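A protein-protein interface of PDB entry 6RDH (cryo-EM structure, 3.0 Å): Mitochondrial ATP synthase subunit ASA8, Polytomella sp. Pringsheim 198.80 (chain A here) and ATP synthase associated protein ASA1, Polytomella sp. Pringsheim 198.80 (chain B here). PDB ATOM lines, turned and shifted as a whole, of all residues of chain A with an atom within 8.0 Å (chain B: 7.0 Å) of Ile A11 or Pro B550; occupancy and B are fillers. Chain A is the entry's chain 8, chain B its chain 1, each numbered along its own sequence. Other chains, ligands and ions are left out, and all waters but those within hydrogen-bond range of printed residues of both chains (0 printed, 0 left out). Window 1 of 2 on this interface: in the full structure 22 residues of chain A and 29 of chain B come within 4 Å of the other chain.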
ATOM      1  N   VAL A   6      26.106 -35.984 -19.128  1.00  0.00           N
ATOM      2  CA  VAL A   6      26.014 -36.080 -17.681  1.00  0.00           C
ATOM      3  C   VAL A   6      26.968 -35.122 -17.008  1.00  0.00           C
ATOM      4  O   VAL A   6      26.880 -34.930 -15.786  1.00  0.00           O
ATOM      5  CB  VAL A   6      26.268 -37.515 -17.186  1.00  0.00           C
ATOM      6  CG1 VAL A   6      25.361 -38.474 -17.916  1.00  0.00           C
ATOM      7  CG2 VAL A   6      27.719 -37.895 -17.370  1.00  0.00           C
ATOM      8  N   TYR A   7      27.884 -34.522 -17.758  1.00  0.00           N
ATOM      9  CA  TYR A   7      28.631 -33.391 -17.251  1.00  0.00           C
ATOM     10  C   TYR A   7      27.845 -32.102 -17.404  1.00  0.00           C
ATOM     11  O   TYR A   7      28.140 -31.127 -16.712  1.00  0.00           O
ATOM     12  CB  TYR A   7      29.978 -33.293 -17.964  1.00  0.00           C
ATOM     13  CG  TYR A   7      30.805 -34.548 -17.837  1.00  0.00           C
ATOM     14  CD1 TYR A   7      31.555 -34.789 -16.700  1.00  0.00           C
ATOM     15  CD2 TYR A   7      30.826 -35.495 -18.846  1.00  0.00           C
ATOM     16  CE1 TYR A   7      32.301 -35.935 -16.573  1.00  0.00           C
ATOM     17  CE2 TYR A   7      31.571 -36.641 -18.730  1.00  0.00           C
ATOM     18  CZ  TYR A   7      32.305 -36.858 -17.592  1.00  0.00           C
ATOM     19  OH  TYR A   7      33.053 -38.004 -17.472  1.00  0.00           O
ATOM     20  N   LEU A   8      26.845 -32.090 -18.277  1.00  0.00           N
ATOM     21  CA  LEU A   8      25.955 -30.957 -18.454  1.00  0.00           C
ATOM     22  C   LEU A   8      24.670 -31.083 -17.659  1.00  0.00           C
ATOM     23  O   LEU A   8      23.734 -30.325 -17.907  1.00  0.00           O
ATOM     24  CB  LEU A   8      25.587 -30.792 -19.922  1.00  0.00           C
ATOM     25  CG  LEU A   8      26.588 -30.525 -21.024  1.00  0.00           C
ATOM     26  CD1 LEU A   8      25.779 -30.271 -22.228  1.00  0.00           C
ATOM     27  CD2 LEU A   8      27.370 -29.324 -20.720  1.00  0.00           C
ATOM     28  N   LYS A   9      24.572 -32.039 -16.749  1.00  0.00           N
ATOM     29  CA  LYS A   9      23.325 -32.247 -16.033  1.00  0.00           C
ATOM     30  C   LYS A   9      23.203 -31.231 -14.911  1.00  0.00           C
ATOM     31  O   LYS A   9      24.112 -31.099 -14.087  1.00  0.00           O
ATOM     32  CB  LYS A   9      23.249 -33.663 -15.481  1.00  0.00           C
ATOM     33  CG  LYS A   9      21.856 -34.082 -15.098  1.00  0.00           C
ATOM     34  CD  LYS A   9      21.814 -35.539 -14.719  1.00  0.00           C
ATOM     35  CE  LYS A   9      22.592 -35.802 -13.442  1.00  0.00           C
ATOM     36  NZ  LYS A   9      21.965 -35.166 -12.253  1.00  0.00           N
ATOM     37  N   ASP A  10      22.090 -30.490 -14.918  1.00  0.00           N
ATOM     38  CA  ASP A  10      21.749 -29.431 -13.968  1.00  0.00           C
ATOM     39  C   ASP A  10      22.754 -28.290 -13.955  1.00  0.00           C
ATOM     40  O   ASP A  10      22.809 -27.533 -12.991  1.00  0.00           O
ATOM     41  CB  ASP A  10      21.572 -29.970 -12.545  1.00  0.00           C
ATOM     42  CG  ASP A  10      20.469 -30.994 -12.437  1.00  0.00           C
ATOM     43  OD1 ASP A  10      19.507 -30.923 -13.227  1.00  0.00           O
ATOM     44  OD2 ASP A  10      20.560 -31.868 -11.553  1.00  0.00           O
ATOM     45  N   ILE A  11      23.545 -28.133 -15.007  1.00  0.00           N
ATOM     46  CA  ILE A  11      24.542 -27.076 -15.075  1.00  0.00           C
ATOM     47  C   ILE A  11      24.239 -26.207 -16.277  1.00  0.00           C
ATOM     48  O   ILE A  11      24.008 -25.003 -16.149  1.00  0.00           O
ATOM     49  CB  ILE A  11      25.964 -27.643 -15.179  1.00  0.00           C
ATOM     50  CG1 ILE A  11      26.302 -28.483 -13.961  1.00  0.00           C
ATOM     51  CG2 ILE A  11      26.944 -26.539 -15.298  1.00  0.00           C
ATOM     52  CD1 ILE A  11      27.609 -29.162 -14.059  1.00  0.00           C
ATOM     53  N   LEU A  12      24.247 -26.816 -17.453  1.00  0.00           N
ATOM     54  CA  LEU A  12      23.995 -26.123 -18.705  1.00  0.00           C
ATOM     55  C   LEU A  12      22.839 -26.812 -19.397  1.00  0.00           C
ATOM     56  O   LEU A  12      22.901 -28.014 -19.654  1.00  0.00           O
ATOM     57  CB  LEU A  12      25.224 -26.143 -19.610  1.00  0.00           C
ATOM     58  CG  LEU A  12      26.363 -25.197 -19.272  1.00  0.00           C
ATOM     59  CD1 LEU A  12      27.557 -25.562 -20.090  1.00  0.00           C
ATOM     60  CD2 LEU A  12      25.952 -23.792 -19.555  1.00  0.00           C
ATOM     61  N   ARG A  13      21.791 -26.064 -19.696  1.00  0.00           N
ATOM     62  CA  ARG A  13      20.692 -26.586 -20.480  1.00  0.00           C
ATOM     63  C   ARG A  13      20.511 -25.725 -21.718  1.00  0.00           C
ATOM     64  O   ARG A  13      20.993 -24.597 -21.788  1.00  0.00           O
ATOM     65  CB  ARG A  13      19.403 -26.634 -19.668  1.00  0.00           C
ATOM     66  CG  ARG A  13      19.545 -27.325 -18.337  1.00  0.00           C
ATOM     67  CD  ARG A  13      18.208 -27.735 -17.802  1.00  0.00           C
ATOM     68  NE  ARG A  13      18.309 -28.435 -16.532  1.00  0.00           N
ATOM     69  CZ  ARG A  13      18.168 -27.859 -15.349  1.00  0.00           C
ATOM     70  NH1 ARG A  13      18.268 -28.579 -14.250  1.00  0.00           N
ATOM     71  NH2 ARG A  13      17.930 -26.567 -15.264  1.00  0.00           N
ATOM     72  N   THR A  14      19.837 -26.279 -22.697  1.00  0.00           N
ATOM     73  CA  THR A  14      19.510 -25.618 -23.945  1.00  0.00           C
ATOM     74  C   THR A  14      18.106 -25.045 -23.858  1.00  0.00           C
ATOM     75  O   THR A  14      17.382 -25.328 -22.900  1.00  0.00           O
ATOM     76  CB  THR A  14      19.634 -26.619 -25.085  1.00  0.00           C
ATOM     77  OG1 THR A  14      18.838 -27.761 -24.777  1.00  0.00           O
ATOM     78  CG2 THR A  14      21.064 -27.023 -25.249  1.00  0.00           C
ATOM     79  N   VAL A  24      11.445 -20.512 -11.575  1.00  0.00           N
ATOM     80  CA  VAL A  24      12.063 -20.942 -10.326  1.00  0.00           C
ATOM     81  C   VAL A  24      11.839 -19.864  -9.278  1.00  0.00           C
ATOM     82  O   VAL A  24      12.243 -18.711  -9.481  1.00  0.00           O
ATOM     83  CB  VAL A  24      13.556 -21.219 -10.511  1.00  0.00           C
ATOM     84  CG1 VAL A  24      14.217 -21.412  -9.182  1.00  0.00           C
ATOM     85  CG2 VAL A  24      13.750 -22.429 -11.352  1.00  0.00           C
ATOM     86  N   GLN B 528      22.839 -21.944 -26.153  1.00  0.00           N
ATOM     87  CA  GLN B 528      22.189 -21.318 -25.012  1.00  0.00           C
ATOM     88  C   GLN B 528      22.372 -19.807 -25.025  1.00  0.00           C
ATOM     89  O   GLN B 528      21.401 -19.056 -24.860  1.00  0.00           O
ATOM     90  CB  GLN B 528      22.736 -21.924 -23.730  1.00  0.00           C
ATOM     91  CG  GLN B 528      22.523 -21.073 -22.531  1.00  0.00           C
ATOM     92  CD  GLN B 528      23.230 -21.610 -21.342  1.00  0.00           C
ATOM     93  OE1 GLN B 528      23.187 -22.802 -21.075  1.00  0.00           O
ATOM     94  NE2 GLN B 528      23.901 -20.737 -20.616  1.00  0.00           N
ATOM     95  N   VAL B 545      15.001 -18.588 -18.827  1.00  0.00           N
ATOM     96  CA  VAL B 545      16.317 -18.190 -18.334  1.00  0.00           C
ATOM     97  C   VAL B 545      16.742 -19.075 -17.172  1.00  0.00           C
ATOM     98  O   VAL B 545      17.881 -19.543 -17.110  1.00  0.00           O
ATOM     99  CB  VAL B 545      16.294 -16.709 -17.931  1.00  0.00           C
ATOM    100  CG1 VAL B 545      17.453 -16.364 -17.060  1.00  0.00           C
ATOM    101  CG2 VAL B 545      16.309 -15.853 -19.131  1.00  0.00           C
ATOM    102  N   ALA B 546      15.828 -19.334 -16.243  1.00  0.00           N
ATOM    103  CA  ALA B 546      16.149 -20.183 -15.106  1.00  0.00           C
ATOM    104  C   ALA B 546      16.233 -21.649 -15.484  1.00  0.00           C
ATOM    105  O   ALA B 546      16.763 -22.445 -14.710  1.00  0.00           O
ATOM    106  CB  ALA B 546      15.113 -19.993 -14.006  1.00  0.00           C
ATOM    107  N   HIS B 547      15.692 -22.028 -16.635  1.00  0.00           N
ATOM    108  CA  HIS B 547      15.865 -23.382 -17.131  1.00  0.00           C
ATOM    109  C   HIS B 547      17.210 -23.535 -17.811  1.00  0.00           C
ATOM    110  O   HIS B 547      17.963 -24.457 -17.503  1.00  0.00           O
ATOM    111  CB  HIS B 547      14.739 -23.724 -18.095  1.00  0.00           C
ATOM    112  CG  HIS B 547      14.856 -25.082 -18.698  1.00  0.00           C
ATOM    113  ND1 HIS B 547      15.267 -25.286 -19.993  1.00  0.00           N
ATOM    114  CD2 HIS B 547      14.616 -26.307 -18.181  1.00  0.00           C
ATOM    115  CE1 HIS B 547      15.278 -26.580 -20.250  1.00  0.00           C
ATOM    116  NE2 HIS B 547      14.888 -27.221 -19.165  1.00  0.00           N
ATOM    117  N   MET B 548      17.522 -22.622 -18.729  1.00  0.00           N
ATOM    118  CA  MET B 548      18.772 -22.663 -19.472  1.00  0.00           C
ATOM    119  C   MET B 548      19.973 -22.470 -18.562  1.00  0.00           C
ATOM    120  O   MET B 548      20.998 -23.131 -18.732  1.00  0.00           O
ATOM    121  CB  MET B 548      18.765 -21.580 -20.536  1.00  0.00           C
ATOM    122  CG  MET B 548      18.451 -22.061 -21.902  1.00  0.00           C
ATOM    123  SD  MET B 548      18.748 -20.754 -23.070  1.00  0.00           S
ATOM    124  CE  MET B 548      17.455 -19.671 -22.563  1.00  0.00           C
ATOM    125  N   ASP B 549      19.872 -21.576 -17.594  1.00  0.00           N
ATOM    126  CA  ASP B 549      20.994 -21.233 -16.726  1.00  0.00           C
ATOM    127  C   ASP B 549      20.542 -21.299 -15.278  1.00  0.00           C
ATOM    128  O   ASP B 549      20.170 -20.280 -14.690  1.00  0.00           O
ATOM    129  CB  ASP B 549      21.536 -19.854 -17.071  1.00  0.00           C
ATOM    130  CG  ASP B 549      23.018 -19.786 -16.940  1.00  0.00           C
ATOM    131  OD1 ASP B 549      23.592 -20.794 -16.507  1.00  0.00           O
ATOM    132  OD2 ASP B 549      23.616 -18.756 -17.297  1.00  0.00           O
ATOM    133  N   PRO B 550      20.558 -22.477 -14.675  1.00  0.00           N
ATOM    134  CA  PRO B 550      20.012 -22.609 -13.325  1.00  0.00           C
ATOM    135  C   PRO B 550      20.957 -22.137 -12.235  1.00  0.00           C
ATOM    136  O   PRO B 550      20.517 -21.602 -11.214  1.00  0.00           O
ATOM    137  CB  PRO B 550      19.737 -24.109 -13.219  1.00  0.00           C
ATOM    138  CG  PRO B 550      20.668 -24.725 -14.138  1.00  0.00           C
ATOM    139  CD  PRO B 550      20.935 -23.777 -15.242  1.00  0.00           C
ATOM    140  N   LEU B 551      22.257 -22.319 -12.431  1.00  0.00           N
ATOM    141  CA  LEU B 551      23.200 -21.938 -11.396  1.00  0.00           C
ATOM    142  C   LEU B 551      23.489 -20.452 -11.409  1.00  0.00           C
ATOM    143  O   LEU B 551      23.848 -19.899 -10.372  1.00  0.00           O
ATOM    144  CB  LEU B 551      24.497 -22.713 -11.544  1.00  0.00           C
ATOM    145  CG  LEU B 551      24.387 -24.221 -11.497  1.00  0.00           C
ATOM    146  CD1 LEU B 551      25.755 -24.782 -11.597  1.00  0.00           C
ATOM    147  CD2 LEU B 551      23.751 -24.636 -10.222  1.00  0.00           C
ATOM    148  N   LEU B 552      23.333 -19.783 -12.548  1.00  0.00           N
ATOM    149  CA  LEU B 552      23.438 -18.331 -12.559  1.00  0.00           C
ATOM    150  C   LEU B 552      22.297 -17.708 -11.786  1.00  0.00           C
ATOM    151  O   LEU B 552      22.501 -16.768 -11.011  1.00  0.00           O
ATOM    152  CB  LEU B 552      23.444 -17.811 -13.988  1.00  0.00           C
ATOM    153  CG  LEU B 552      23.570 -16.303 -14.131  1.00  0.00           C
ATOM    154  CD1 LEU B 552      24.868 -15.853 -13.543  1.00  0.00           C
ATOM    155  CD2 LEU B 552      23.478 -15.888 -15.565  1.00  0.00           C
ATOM    156  N   ILE B 553      21.089 -18.236 -11.972  1.00  0.00           N
ATOM    157  CA  ILE B 553      19.930 -17.806 -11.204  1.00  0.00           C
ATOM    158  C   ILE B 553      20.103 -18.147  -9.735  1.00  0.00           C
ATOM    159  O   ILE B 553      19.718 -17.364  -8.866  1.00  0.00           O
ATOM    160  CB  ILE B 553      18.674 -18.437 -11.828  1.00  0.00           C
ATOM    161  CG1 ILE B 553      18.375 -17.781 -13.173  1.00  0.00           C
ATOM    162  CG2 ILE B 553      17.490 -18.358 -10.940  1.00  0.00           C
ATOM    163  CD1 ILE B 553      18.381 -16.292 -13.172  1.00  0.00           C
ATOM    164  N   LYS B 554      20.768 -19.259  -9.432  1.00  0.00           N
ATOM    165  CA  LYS B 554      21.059 -19.615  -8.047  1.00  0.00           C
ATOM    166  C   LYS B 554      22.011 -18.627  -7.386  1.00  0.00           C
ATOM    167  O   LYS B 554      21.789 -18.214  -6.243  1.00  0.00           O
ATOM    168  CB  LYS B 554      21.637 -21.018  -8.003  1.00  0.00           C
ATOM    169  CG  LYS B 554      22.149 -21.425  -6.676  1.00  0.00           C
ATOM    170  CD  LYS B 554      22.713 -22.795  -6.729  1.00  0.00           C
ATOM    171  CE  LYS B 554      22.976 -23.272  -5.351  1.00  0.00           C
ATOM    172  NZ  LYS B 554      23.559 -24.621  -5.386  1.00  0.00           N
ATOM    173  N   LYS B 555      23.049 -18.203  -8.097  1.00  0.00           N
ATOM    174  CA  LYS B 555      23.996 -17.251  -7.529  1.00  0.00           C
ATOM    175  C   LYS B 555      23.397 -15.858  -7.399  1.00  0.00           C
ATOM    176  O   LYS B 555      23.666 -15.146  -6.424  1.00  0.00           O
ATOM    177  CB  LYS B 555      25.242 -17.203  -8.388  1.00  0.00           C
ATOM    178  CG  LYS B 555      25.969 -18.489  -8.420  1.00  0.00           C
ATOM    179  CD  LYS B 555      26.990 -18.475  -9.488  1.00  0.00           C
ATOM    180  CE  LYS B 555      27.646 -19.793  -9.555  1.00  0.00           C
ATOM    181  NZ  LYS B 555      28.869 -19.738 -10.358  1.00  0.00           N
ATOM    182  N   ASP B 557      20.220 -15.262  -6.930  1.00  0.00           N
ATOM    183  CA  ASP B 557      19.329 -15.376  -5.788  1.00  0.00           C
ATOM    184  C   ASP B 557      20.088 -15.434  -4.473  1.00  0.00           C
ATOM    185  O   ASP B 557      19.539 -15.060  -3.439  1.00  0.00           O
ATOM    186  CB  ASP B 557      18.458 -16.609  -5.940  1.00  0.00           C
ATOM    187  CG  ASP B 557      17.436 -16.452  -7.019  1.00  0.00           C
ATOM    188  OD1 ASP B 557      17.377 -15.359  -7.602  1.00  0.00           O
ATOM    189  OD2 ASP B 557      16.690 -17.412  -7.289  1.00  0.00           O
ATOM    190  N   HIS B 590      30.524 -21.510 -13.663  1.00  0.00           N
ATOM    191  CA  HIS B 590      29.965 -22.840 -13.804  1.00  0.00           C
ATOM    192  C   HIS B 590      29.804 -23.250 -15.248  1.00  0.00           C
ATOM    193  O   HIS B 590      29.363 -24.367 -15.507  1.00  0.00           O
ATOM    194  CB  HIS B 590      28.608 -22.910 -13.120  1.00  0.00           C
ATOM    195  CG  HIS B 590      27.668 -21.839 -13.558  1.00  0.00           C
ATOM    196  ND1 HIS B 590      26.676 -22.060 -14.481  1.00  0.00           N
ATOM    197  CD2 HIS B 590      27.579 -20.536 -13.214  1.00  0.00           C
ATOM    198  CE1 HIS B 590      26.012 -20.940 -14.682  1.00  0.00           C
ATOM    199  NE2 HIS B 590      26.546 -19.998 -13.931  1.00  0.00           N
ATOM    200  N   HIS B 591      30.114 -22.371 -16.193  1.00  0.00           N
ATOM    201  CA  HIS B 591      30.051 -22.749 -17.592  1.00  0.00           C
ATOM    202  C   HIS B 591      31.209 -23.648 -17.967  1.00  0.00           C
ATOM    203  O   HIS B 591      31.075 -24.486 -18.860  1.00  0.00           O
ATOM    204  CB  HIS B 591      30.045 -21.506 -18.459  1.00  0.00           C
ATOM    205  CG  HIS B 591      28.745 -20.778 -18.444  1.00  0.00           C
ATOM    206  ND1 HIS B 591      28.560 -19.572 -19.074  1.00  0.00           N
ATOM    207  CD2 HIS B 591      27.560 -21.097 -17.885  1.00  0.00           C
ATOM    208  CE1 HIS B 591      27.316 -19.174 -18.896  1.00  0.00           C
ATOM    209  NE2 HIS B 591      26.688 -20.081 -18.175  1.00  0.00           N
ATOM    210  N   PHE B 592      32.344 -23.488 -17.309  1.00  0.00           N
ATOM    211  CA  PHE B 592      33.505 -24.326 -17.532  1.00  0.00           C
ATOM    212  C   PHE B 592      33.566 -25.497 -16.578  1.00  0.00           C
ATOM    213  O   PHE B 592      34.554 -26.225 -16.588  1.00  0.00           O
ATOM    214  CB  PHE B 592      34.780 -23.505 -17.398  1.00  0.00           C
ATOM    215  CG  PHE B 592      34.755 -22.230 -18.162  1.00  0.00           C
ATOM    216  CD1 PHE B 592      35.040 -22.212 -19.507  1.00  0.00           C
ATOM    217  CD2 PHE B 592      34.454 -21.048 -17.535  1.00  0.00           C
ATOM    218  CE1 PHE B 592      35.016 -21.042 -20.206  1.00  0.00           C
ATOM    219  CE2 PHE B 592      34.432 -19.879 -18.235  1.00  0.00           C
ATOM    220  CZ  PHE B 592      34.714 -19.879 -19.568  1.00  0.00           C
ATOM    221  N   LEU B 593      32.572 -25.678 -15.743  1.00  0.00           N
ATOM    222  CA  LEU B 593      32.500 -26.854 -14.889  1.00  0.00           C
ATOM    223  C   LEU B 593      32.282 -28.176 -15.636  1.00  0.00           C
ATOM    224  O   LEU B 593      32.903 -29.170 -15.232  1.00  0.00           O
ATOM    225  CB  LEU B 593      31.421 -26.664 -13.827  1.00  0.00           C
ATOM    226  CG  LEU B 593      31.250 -27.792 -12.826  1.00  0.00           C
ATOM    227  CD1 LEU B 593      32.512 -27.965 -12.056  1.00  0.00           C
ATOM    228  CD2 LEU B 593      30.137 -27.484 -11.913  1.00  0.00           C
ATOM    229  N   PRO B 594      31.438 -28.277 -16.689  1.00  0.00           N
ATOM    230  CA  PRO B 594      31.395 -29.551 -17.429  1.00  0.00           C
ATOM    231  C   PRO B 594      32.709 -29.938 -18.071  1.00  0.00           C
ATOM    232  O   PRO B 594      33.092 -31.113 -18.031  1.00  0.00           O
ATOM    233  CB  PRO B 594      30.323 -29.289 -18.486  1.00  0.00           C
ATOM    234  CG  PRO B 594      29.471 -28.329 -17.892  1.00  0.00           C
ATOM    235  CD  PRO B 594      30.340 -27.412 -17.164  1.00  0.00           C
ATOM    236  N   ARG B 597      35.241 -30.986 -15.242  1.00  0.00           N
ATOM    237  CA  ARG B 597      34.882 -32.286 -14.691  1.00  0.00           C
ATOM    238  C   ARG B 597      35.201 -33.411 -15.668  1.00  0.00           C
ATOM    239  O   ARG B 597      35.694 -34.470 -15.262  1.00  0.00           O
ATOM    240  CB  ARG B 597      33.411 -32.305 -14.322  1.00  0.00           C
ATOM    241  CG  ARG B 597      33.136 -31.667 -13.015  1.00  0.00           C
ATOM    242  CD  ARG B 597      31.659 -31.564 -12.777  1.00  0.00           C
ATOM    243  NE  ARG B 597      31.003 -32.855 -12.731  1.00  0.00           N
ATOM    244  CZ  ARG B 597      31.002 -33.651 -11.672  1.00  0.00           C
ATOM    245  NH1 ARG B 597      31.639 -33.303 -10.565  1.00  0.00           N
ATOM    246  NH2 ARG B 597      30.366 -34.807 -11.727  1.00  0.00           N
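NH2 of Arg A13 lies within hydrogen-bond range of O of His B547 (3.1 Å).
OE1 of Gln B528 sits close to O of Arg A13, at 2.9 Å.
O of Met B548 lies within hydrogen-bond range of N of Arg A13.
The side-chain carboxylate (OD2) of Asp B549 sits at hydrogen-bond distance from a ring nitrogen (NE2) of His B591 (3.5 Å).
The side-chain carboxylate (OD2) of Asp A10 lies within salt-bridge range of the side-chain amino group (NZ) of Lys A9, at 3.7 Å.
The side-chain carboxylate of Asp A10 lies within salt-bridge range of the guanidinium group of Arg A13 (2.8 Å).
OE1 of Gln B528 lies close to O of Met B548 (3.2 Å).
Tyr A7 touches Pro B594.
Leu A8 touches Pro B594.
O of Asp A10 touches CG of Pro B550 (3.7 Å).
CG of Leu B551 touches O of Asp A10, 3.96 Å away.
Ile A11 touches Leu B593.
Gln B528 touches Leu A12 (OE1 to CD2, 3.3 Å).
CD2 of His B591 touches CD2 of Leu A12, 3.6 Å away.
ND1 of His B547 touches O of Thr A14 (3.6 Å).
Thr A14 touches Met B548.
CB of Ala B546 touches CG2 of Val A24, at 3.9 Å.
Ile A11 touches just these residues of chain B: Pro B550 (3.4 Å), His B590 (3.3 Å), Leu B593 (3.7 Å) and Pro B594 (3.97 Å).
Of chain A, only Asp A10 (3.7 Å), Ile A11 (3.4 Å) and Arg A13 (3.5 Å) come within 4 Å of Pro B550.
Of the printed residues of chain A, Met B548 touches Arg A13 (3.2 Å) and Thr A14 (3.6 Å).
Of the printed residues of chain A, His B547 touches Arg A13 (3.1 Å) and Thr A14 (3.6 Å).
Of the printed residues of chain A, Arg B597 touches Tyr A7.
Lys B555 touches none of the printed residues of chain A.
The nearest residue of chain A that does not touch Pro B550 is Leu A12 (5.0 Å).
Hydrophobic or aromatic side chains of chain A within 4 Å of the printed part of chain B: Tyr A7, Leu A8, Ile A11, Leu A12 and Val A24.
Along chain A the printed residues that touch a printed residue of chain B span positions 7 to 24.
Printed residues of chain B that touch a printed residue of chain A: Gln B528, Ala B546, His B547, Met B548, Pro B550, Leu B551, His B590, His B591, Leu B593, Pro B594 and Arg B597.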
